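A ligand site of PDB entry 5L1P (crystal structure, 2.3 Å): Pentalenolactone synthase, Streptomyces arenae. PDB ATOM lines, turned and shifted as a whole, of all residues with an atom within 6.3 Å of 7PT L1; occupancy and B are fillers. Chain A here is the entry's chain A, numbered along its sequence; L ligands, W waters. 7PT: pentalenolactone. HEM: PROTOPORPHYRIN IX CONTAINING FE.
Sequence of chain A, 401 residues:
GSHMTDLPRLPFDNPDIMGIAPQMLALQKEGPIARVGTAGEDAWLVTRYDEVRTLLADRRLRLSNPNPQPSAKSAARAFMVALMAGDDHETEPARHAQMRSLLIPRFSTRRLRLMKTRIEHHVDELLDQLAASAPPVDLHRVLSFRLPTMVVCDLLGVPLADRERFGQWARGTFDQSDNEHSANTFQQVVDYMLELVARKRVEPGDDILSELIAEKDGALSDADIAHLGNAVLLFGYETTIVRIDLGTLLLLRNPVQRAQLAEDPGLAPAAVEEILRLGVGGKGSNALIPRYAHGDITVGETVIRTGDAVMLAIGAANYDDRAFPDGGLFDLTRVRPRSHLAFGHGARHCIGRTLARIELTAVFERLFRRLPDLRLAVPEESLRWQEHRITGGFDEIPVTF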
ATOM      1  N   ARG A  77       7.685 -31.264  -3.424  1.00  0.00           N
ATOM      2  CA  ARG A  77       7.332 -31.382  -4.831  1.00  0.00           C
ATOM      3  C   ARG A  77       6.754 -32.765  -5.135  1.00  0.00           C
ATOM      4  O   ARG A  77       5.834 -32.895  -5.955  1.00  0.00           O
ATOM      5  CB  ARG A  77       8.577 -31.083  -5.685  1.00  0.00           C
ATOM      6  CG  ARG A  77       8.300 -30.958  -7.169  1.00  0.00           C
ATOM      7  CD  ARG A  77       7.314 -29.831  -7.483  1.00  0.00           C
ATOM      8  NE  ARG A  77       7.873 -28.482  -7.393  1.00  0.00           N
ATOM      9  CZ  ARG A  77       7.267 -27.392  -7.878  1.00  0.00           C
ATOM     10  NH1 ARG A  77       6.090 -27.512  -8.480  1.00  0.00           N
ATOM     11  NH2 ARG A  77       7.827 -26.202  -7.767  1.00  0.00           N
ATOM     12  N   MET A  80       3.169 -32.693  -4.073  1.00  0.00           N
ATOM     13  CA  MET A  80       2.412 -31.887  -5.033  1.00  0.00           C
ATOM     14  C   MET A  80       2.132 -32.665  -6.305  1.00  0.00           C
ATOM     15  O   MET A  80       0.992 -32.695  -6.802  1.00  0.00           O
ATOM     16  CB  MET A  80       3.148 -30.595  -5.349  1.00  0.00           C
ATOM     17  CG  MET A  80       2.479 -29.795  -6.470  1.00  0.00           C
ATOM     18  SD  MET A  80       3.017 -28.083  -6.496  1.00  0.00           S
ATOM     19  CE  MET A  80       2.198 -27.475  -4.999  1.00  0.00           C
ATOM     20  N   MET A  84      -1.533 -34.326  -7.965  1.00  0.00           N
ATOM     21  CA  MET A  84      -1.995 -33.962  -9.292  1.00  0.00           C
ATOM     22  C   MET A  84      -2.042 -35.153 -10.249  1.00  0.00           C
ATOM     23  O   MET A  84      -2.190 -34.944 -11.458  1.00  0.00           O
ATOM     24  CB  MET A  84      -1.105 -32.860  -9.865  1.00  0.00           C
ATOM     25  CG  MET A  84      -1.090 -31.585  -8.992  1.00  0.00           C
ATOM     26  SD  MET A  84       0.028 -30.282  -9.586  1.00  0.00           S
ATOM     27  CE  MET A  84      -0.720 -29.873 -11.165  1.00  0.00           C
ATOM     28  N   PHE A 235      -4.545 -27.331  -2.202  1.00  0.00           N
ATOM     29  CA  PHE A 235      -4.546 -26.321  -3.251  1.00  0.00           C
ATOM     30  C   PHE A 235      -5.644 -25.251  -3.055  1.00  0.00           C
ATOM     31  O   PHE A 235      -5.593 -24.199  -3.708  1.00  0.00           O
ATOM     32  CB  PHE A 235      -4.727 -26.966  -4.653  1.00  0.00           C
ATOM     33  CG  PHE A 235      -3.708 -28.073  -4.958  1.00  0.00           C
ATOM     34  CD1 PHE A 235      -2.450 -28.075  -4.378  1.00  0.00           C
ATOM     35  CD2 PHE A 235      -4.044 -29.110  -5.821  1.00  0.00           C
ATOM     36  CE1 PHE A 235      -1.524 -29.084  -4.660  1.00  0.00           C
ATOM     37  CE2 PHE A 235      -3.138 -30.133  -6.107  1.00  0.00           C
ATOM     38  CZ  PHE A 235      -1.874 -30.123  -5.527  1.00  0.00           C
ATOM     39  N   THR A 239      -2.840 -20.478  -2.225  1.00  0.00           N
ATOM     40  CA  THR A 239      -2.611 -19.567  -3.347  1.00  0.00           C
ATOM     41  C   THR A 239      -3.564 -18.381  -3.296  1.00  0.00           C
ATOM     42  O   THR A 239      -3.168 -17.249  -3.625  1.00  0.00           O
ATOM     43  CB  THR A 239      -2.758 -20.282  -4.693  1.00  0.00           C
ATOM     44  OG1 THR A 239      -4.067 -20.848  -4.785  1.00  0.00           O
ATOM     45  CG2 THR A 239      -1.703 -21.376  -4.868  1.00  0.00           C
ATOM     46  N   ARG A 243      -2.706 -14.407  -3.207  1.00  0.00           N
ATOM     47  CA  ARG A 243      -3.243 -13.426  -4.159  1.00  0.00           C
ATOM     48  C   ARG A 243      -3.936 -12.266  -3.447  1.00  0.00           C
ATOM     49  O   ARG A 243      -3.950 -11.150  -3.976  1.00  0.00           O
ATOM     50  CB  ARG A 243      -4.185 -14.112  -5.159  1.00  0.00           C
ATOM     51  CG  ARG A 243      -3.469 -15.051  -6.132  1.00  0.00           C
ATOM     52  CD  ARG A 243      -2.028 -14.582  -6.410  1.00  0.00           C
ATOM     53  NE  ARG A 243      -1.285 -15.497  -7.272  1.00  0.00           N
ATOM     54  CZ  ARG A 243      -0.713 -16.621  -6.854  1.00  0.00           C
ATOM     55  NH1 ARG A 243      -0.795 -16.987  -5.585  1.00  0.00           N
ATOM     56  NH2 ARG A 243      -0.054 -17.390  -7.714  1.00  0.00           N
ATOM     57  N   SER A 285       9.315 -18.126  -8.137  1.00  0.00           N
ATOM     58  CA  SER A 285       9.483 -19.549  -8.411  1.00  0.00           C
ATOM     59  C   SER A 285       8.157 -20.276  -8.557  1.00  0.00           C
ATOM     60  O   SER A 285       8.058 -21.231  -9.326  1.00  0.00           O
ATOM     61  CB  SER A 285      10.291 -20.191  -7.303  1.00  0.00           C
ATOM     62  OG  SER A 285      11.664 -19.879  -7.467  1.00  0.00           O
ATOM     63  N   ASN A 286       7.136 -19.868  -7.801  1.00  0.00           N
ATOM     64  CA  ASN A 286       5.806 -20.443  -7.961  1.00  0.00           C
ATOM     65  C   ASN A 286       5.114 -20.006  -9.253  1.00  0.00           C
ATOM     66  O   ASN A 286       4.097 -20.602  -9.613  1.00  0.00           O
ATOM     67  CB  ASN A 286       4.903 -20.080  -6.775  1.00  0.00           C
ATOM     68  CG  ASN A 286       4.704 -18.585  -6.651  1.00  0.00           C
ATOM     69  OD1 ASN A 286       5.655 -17.811  -6.695  1.00  0.00           O
ATOM     70  ND2 ASN A 286       3.451 -18.170  -6.484  1.00  0.00           N
ATOM     71  N   ALA A 287       5.624 -18.985  -9.942  1.00  0.00           N
ATOM     72  CA  ALA A 287       5.078 -18.577 -11.236  1.00  0.00           C
ATOM     73  C   ALA A 287       5.740 -19.323 -12.391  1.00  0.00           C
ATOM     74  O   ALA A 287       5.808 -18.790 -13.498  1.00  0.00           O
ATOM     75  CB  ALA A 287       5.212 -17.063 -11.422  1.00  0.00           C
ATOM     76  N   LEU A 288       6.263 -20.518 -12.133  1.00  0.00           N
ATOM     77  CA  LEU A 288       6.794 -21.420 -13.147  1.00  0.00           C
ATOM     78  C   LEU A 288       6.001 -22.712 -13.079  1.00  0.00           C
ATOM     79  O   LEU A 288       5.938 -23.346 -12.021  1.00  0.00           O
ATOM     80  CB  LEU A 288       8.274 -21.724 -12.921  1.00  0.00           C
ATOM     81  CG  LEU A 288       9.277 -20.574 -12.900  1.00  0.00           C
ATOM     82  CD1 LEU A 288      10.640 -21.101 -12.466  1.00  0.00           C
ATOM     83  CD2 LEU A 288       9.346 -19.905 -14.268  1.00  0.00           C
ATOM     84  N   ILE A 289       5.422 -23.114 -14.210  1.00  0.00           N
ATOM     85  CA  ILE A 289       4.734 -24.397 -14.314  1.00  0.00           C
ATOM     86  C   ILE A 289       5.743 -25.417 -14.872  1.00  0.00           C
ATOM     87  O   ILE A 289       6.253 -25.200 -15.988  1.00  0.00           O
ATOM     88  CB  ILE A 289       3.496 -24.295 -15.196  1.00  0.00           C
ATOM     89  CG1 ILE A 289       2.395 -23.497 -14.478  1.00  0.00           C
ATOM     90  CG2 ILE A 289       3.011 -25.686 -15.634  1.00  0.00           C
ATOM     91  CD1 ILE A 289       1.118 -23.302 -15.341  1.00  0.00           C
ATOM     92  N   PRO A 290       6.026 -26.495 -14.157  1.00  0.00           N
ATOM     93  CA  PRO A 290       7.011 -27.482 -14.637  1.00  0.00           C
ATOM     94  C   PRO A 290       6.403 -28.578 -15.499  1.00  0.00           C
ATOM     95  O   PRO A 290       5.288 -29.050 -15.249  1.00  0.00           O
ATOM     96  CB  PRO A 290       7.553 -28.062 -13.321  1.00  0.00           C
ATOM     97  CG  PRO A 290       6.325 -28.042 -12.420  1.00  0.00           C
ATOM     98  CD  PRO A 290       5.521 -26.822 -12.809  1.00  0.00           C
ATOM     99  N   ARG A 291       7.140 -28.991 -16.538  1.00  0.00           N
ATOM    100  CA  ARG A 291       6.687 -30.065 -17.422  1.00  0.00           C
ATOM    101  C   ARG A 291       7.899 -30.842 -17.902  1.00  0.00           C
ATOM    102  O   ARG A 291       9.040 -30.374 -17.818  1.00  0.00           O
ATOM    103  CB  ARG A 291       5.936 -29.547 -18.656  1.00  0.00           C
ATOM    104  CG  ARG A 291       4.634 -28.823 -18.400  1.00  0.00           C
ATOM    105  CD  ARG A 291       3.528 -29.777 -18.008  1.00  0.00           C
ATOM    106  NE  ARG A 291       2.244 -29.079 -17.922  1.00  0.00           N
ATOM    107  CZ  ARG A 291       1.646 -28.702 -16.797  1.00  0.00           C
ATOM    108  NH1 ARG A 291       2.205 -28.955 -15.607  1.00  0.00           N
ATOM    109  NH2 ARG A 291       0.481 -28.066 -16.860  1.00  0.00           N
ATOM    110  N   ILE A 314       4.764 -18.633 -16.480  1.00  0.00           N
ATOM    111  CA  ILE A 314       3.477 -17.947 -16.640  1.00  0.00           C
ATOM    112  C   ILE A 314       3.528 -16.540 -16.064  1.00  0.00           C
ATOM    113  O   ILE A 314       2.775 -15.667 -16.494  1.00  0.00           O
ATOM    114  CB  ILE A 314       2.342 -18.770 -16.013  1.00  0.00           C
ATOM    115  CG1 ILE A 314       2.571 -18.955 -14.501  1.00  0.00           C
ATOM    116  CG2 ILE A 314       2.179 -20.103 -16.743  1.00  0.00           C
ATOM    117  CD1 ILE A 314       1.402 -19.644 -13.775  1.00  0.00           C
ATOM    118  N   ALA A 342      -2.303 -16.929 -15.307  1.00  0.00           N
ATOM    119  CA  ALA A 342      -2.067 -17.172 -13.886  1.00  0.00           C
ATOM    120  C   ALA A 342      -2.802 -18.397 -13.357  1.00  0.00           C
ATOM    121  O   ALA A 342      -2.420 -18.909 -12.295  1.00  0.00           O
ATOM    122  CB  ALA A 342      -2.441 -15.938 -13.053  1.00  0.00           C
ATOM    123  N   ILE A 390       6.818 -23.986  -1.985  1.00  0.00           N
ATOM    124  CA  ILE A 390       6.436 -24.050  -3.391  1.00  0.00           C
ATOM    125  C   ILE A 390       5.471 -22.919  -3.724  1.00  0.00           C
ATOM    126  O   ILE A 390       5.555 -22.305  -4.794  1.00  0.00           O
ATOM    127  CB  ILE A 390       5.832 -25.422  -3.733  1.00  0.00           C
ATOM    128  CG1 ILE A 390       6.858 -26.525  -3.606  1.00  0.00           C
ATOM    129  CG2 ILE A 390       5.244 -25.396  -5.138  1.00  0.00           C
ATOM    130  CD1 ILE A 390       6.304 -27.883  -3.964  1.00  0.00           C
ATOM    131  N   THR A 391       4.557 -22.621  -2.792  1.00  0.00           N
ATOM    132  CA  THR A 391       3.516 -21.607  -2.935  1.00  0.00           C
ATOM    133  C   THR A 391       3.977 -20.219  -2.492  1.00  0.00           C
ATOM    134  O   THR A 391       3.229 -19.240  -2.687  1.00  0.00           O
ATOM    135  CB  THR A 391       2.250 -22.059  -2.170  1.00  0.00           C
ATOM    136  OG1 THR A 391       2.607 -22.529  -0.856  1.00  0.00           O
ATOM    137  CG2 THR A 391       1.559 -23.210  -2.910  1.00  0.00           C
ATOM    138  N   GLY A 392       5.183 -20.092  -1.932  1.00  0.00           N
ATOM    139  CA  GLY A 392       5.743 -18.780  -1.642  1.00  0.00           C
ATOM    140  C   GLY A 392       4.957 -18.031  -0.584  1.00  0.00           C
ATOM    141  O   GLY A 392       4.703 -18.540   0.510  1.00  0.00           O
HETATM  142  C1  7PT L   1      -1.155 -24.706  -8.590  1.00  0.00           C
HETATM  143  O1  7PT L   1       2.152 -24.651 -11.092  1.00  0.00           O
HETATM  144  C2  7PT L   1      -0.444 -25.901  -8.312  1.00  0.00           C
HETATM  145  C3  7PT L   1       0.894 -25.757  -8.390  1.00  0.00           C
HETATM  146  C4  7PT L   1       1.238 -24.413  -8.677  1.00  0.00           C
HETATM  147  C5  7PT L   1       1.540 -23.598  -7.392  1.00  0.00           C
HETATM  148  C15 7PT L   1      -1.138 -27.248  -8.035  1.00  0.00           C
HETATM  149  C14 7PT L   1      -1.859 -24.218  -7.323  1.00  0.00           C
HETATM  150  C7  7PT L   1       0.036 -22.433  -8.669  1.00  0.00           C
HETATM  151  C12 7PT L   1       3.074 -23.419  -7.291  1.00  0.00           C
HETATM  152  C10 7PT L   1       2.498 -23.249 -10.734  1.00  0.00           C
HETATM  153  C13 7PT L   1       1.192 -21.182  -6.964  1.00  0.00           C
HETATM  154  C11 7PT L   1       3.566 -24.882  -9.168  1.00  0.00           C
HETATM  155  C6  7PT L   1       0.921 -22.330  -7.635  1.00  0.00           C
HETATM  156  C8  7PT L   1      -0.049 -23.772  -9.192  1.00  0.00           C
HETATM  157  C9  7PT L   1       2.390 -24.347  -9.711  1.00  0.00           C
HETATM  158  O4  7PT L   1       1.957 -21.131  -5.980  1.00  0.00           O
HETATM  159  O2  7PT L   1       4.207 -25.710  -9.811  1.00  0.00           O
HETATM  160  O5  7PT L   1       0.650 -20.092  -7.267  1.00  0.00           O
HETATM  161  O3  7PT L   1       3.868 -24.505  -7.882  1.00  0.00           O
HETATM  162  CHA HEM L   2      -4.128 -26.106 -10.909  1.00  0.00           C
HETATM  163  CHB HEM L   2      -3.279 -21.447  -9.899  1.00  0.00           C
HETATM  164  CHC HEM L   2      -6.904 -21.410  -6.665  1.00  0.00           C
HETATM  165  CHD HEM L   2      -7.476 -26.155  -7.367  1.00  0.00           C
HETATM  166  C1A HEM L   2      -3.639 -24.841 -10.983  1.00  0.00           C
HETATM  167  C2A HEM L   2      -2.647 -24.353 -11.922  1.00  0.00           C
HETATM  168  C3A HEM L   2      -2.410 -23.065 -11.627  1.00  0.00           C
HETATM  169  C4A HEM L   2      -3.241 -22.695 -10.499  1.00  0.00           C
HETATM  170  CMA HEM L   2      -1.431 -22.121 -12.361  1.00  0.00           C
HETATM  171  CAA HEM L   2      -1.988 -25.177 -13.066  1.00  0.00           C
HETATM  172  CBA HEM L   2      -0.778 -25.979 -12.564  1.00  0.00           C
HETATM  173  CGA HEM L   2      -0.229 -26.810 -13.716  1.00  0.00           C
HETATM  174  O1A HEM L   2      -0.712 -26.626 -14.867  1.00  0.00           O
HETATM  175  O2A HEM L   2       0.695 -27.647 -13.484  1.00  0.00           O
HETATM  176  C1B HEM L   2      -4.169 -21.025  -8.944  1.00  0.00           C
HETATM  177  C2B HEM L   2      -4.259 -19.689  -8.373  1.00  0.00           C
HETATM  178  C3B HEM L   2      -5.248 -19.719  -7.470  1.00  0.00           C
HETATM  179  C4B HEM L   2      -5.833 -21.034  -7.452  1.00  0.00           C
HETATM  180  CMB HEM L   2      -3.325 -18.502  -8.748  1.00  0.00           C
HETATM  181  CAB HEM L   2      -5.829 -18.599  -6.573  1.00  0.00           C
HETATM  182  CBB HEM L   2      -5.865 -17.329  -6.997  1.00  0.00           C
HETATM  183  C1C HEM L   2      -7.433 -22.677  -6.562  1.00  0.00           C
HETATM  184  C2C HEM L   2      -8.578 -23.087  -5.769  1.00  0.00           C
HETATM  185  C3C HEM L   2      -8.727 -24.416  -5.983  1.00  0.00           C
HETATM  186  C4C HEM L   2      -7.679 -24.862  -6.891  1.00  0.00           C
HETATM  187  CMC HEM L   2      -9.452 -22.120  -4.894  1.00  0.00           C
HETATM  188  CAC HEM L   2      -9.767 -25.426  -5.420  1.00  0.00           C
HETATM  189  CBC HEM L   2     -10.632 -25.189  -4.436  1.00  0.00           C
HETATM  190  C1D HEM L   2      -6.608 -26.561  -8.352  1.00  0.00           C
HETATM  191  C2D HEM L   2      -6.403 -27.925  -8.811  1.00  0.00           C
HETATM  192  C3D HEM L   2      -5.471 -27.909  -9.782  1.00  0.00           C
HETATM  193  C4D HEM L   2      -5.049 -26.544  -9.975  1.00  0.00           C
HETATM  194  CMD HEM L   2      -7.127 -29.172  -8.286  1.00  0.00           C
HETATM  195  CAD HEM L   2      -4.949 -29.121 -10.570  1.00  0.00           C
HETATM  196  CBD HEM L   2      -5.489 -29.097 -12.007  1.00  0.00           C
HETATM  197  CGD HEM L   2      -4.943 -30.287 -12.741  1.00  0.00           C
HETATM  198  O1D HEM L   2      -5.682 -30.852 -13.581  1.00  0.00           O
HETATM  199  O2D HEM L   2      -3.778 -30.714 -12.502  1.00  0.00           O
HETATM  200  NA  HEM L   2      -3.985 -23.804 -10.129  1.00  0.00           N
HETATM  201  NB  HEM L   2      -5.134 -21.817  -8.357  1.00  0.00           N
HETATM  202  NC  HEM L   2      -6.914 -23.769  -7.229  1.00  0.00           N
HETATM  203  ND  HEM L   2      -5.757 -25.749  -9.089  1.00  0.00           N
HETATM  204 FE   HEM L   2      -5.678 -23.695  -8.936  1.00  0.00          FE
HETATM  205  O   HOH W   1      -4.337 -23.423  -5.639  1.00  0.00           O
HETATM  206  O   HOH W   2       6.968 -24.091  -9.576  1.00  0.00           O
HETATM  207  O   HOH W   3       0.933 -18.970  -4.210  1.00  0.00           O
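Water W3 lies within hydrogen-bond range of the backbone carbonyl oxygen (O) of Thr 391, the guanidinium group (NH1) of Arg 243, an oxygen (O4) of 7PT L1 and the side-chain amide nitrogen (ND2) of Asn 286. Water W1 bridges the backbone carbonyl oxygen of Phe 235 (2.4 Å) and the side-chain hydroxyl of Thr 239 (2.7 Å).
The guanidinium group (NH1) of Arg 243 sits at hydrogen-bond distance from the backbone carbonyl oxygen (O) of Thr 239, 3.1 Å away. The guanidinium group (NH1) of Arg 77 is in hydrogen-bond range of the side-chain sulfur (SD) of Met 80, at 3.7 Å.
Met 80 touches 7PT L1 (SD to C3, 3.7 Å). SD of Met 84 touches C15 of 7PT L1 (3.6 Å). CE1 of Phe 235 touches C15 of 7PT L1, 3.9 Å away. CG2 of Thr 239 touches C13 of 7PT L1, at 3.6 Å. O of Leu 288 touches O2 of 7PT L1, at 3.7 Å. CG1 of Ile 289 touches O1 of 7PT L1 (3.6 Å). Pro 290 touches 7PT L1 (CD to O2, 3.5 Å). Ile 390 touches 7PT L1. Thr 391 touches 7PT L1. Within 4 Å of 7PT L1: Arg 77, Met 80, Met 84, Phe 235, Thr 239, Arg 243, Asn 286, Leu 288, Ile 289, Pro 290, Ile 390 and Thr 391.
O5 of 7PT L1 is in salt-bridge range of NH2 of Arg 243 (2.8 Å). The guanidinium group (NH1) of Arg 77 lies within hydrogen-bond range of an oxygen (O2) of 7PT L1 (2.9 Å). The side-chain amide nitrogen (ND2) of Asn 286 sits close to an oxygen (O4) of 7PT L1 (3.4 Å). The guanidinium group of Arg 291 lies within salt-bridge range of an oxygen (O1A) of HEM L2.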
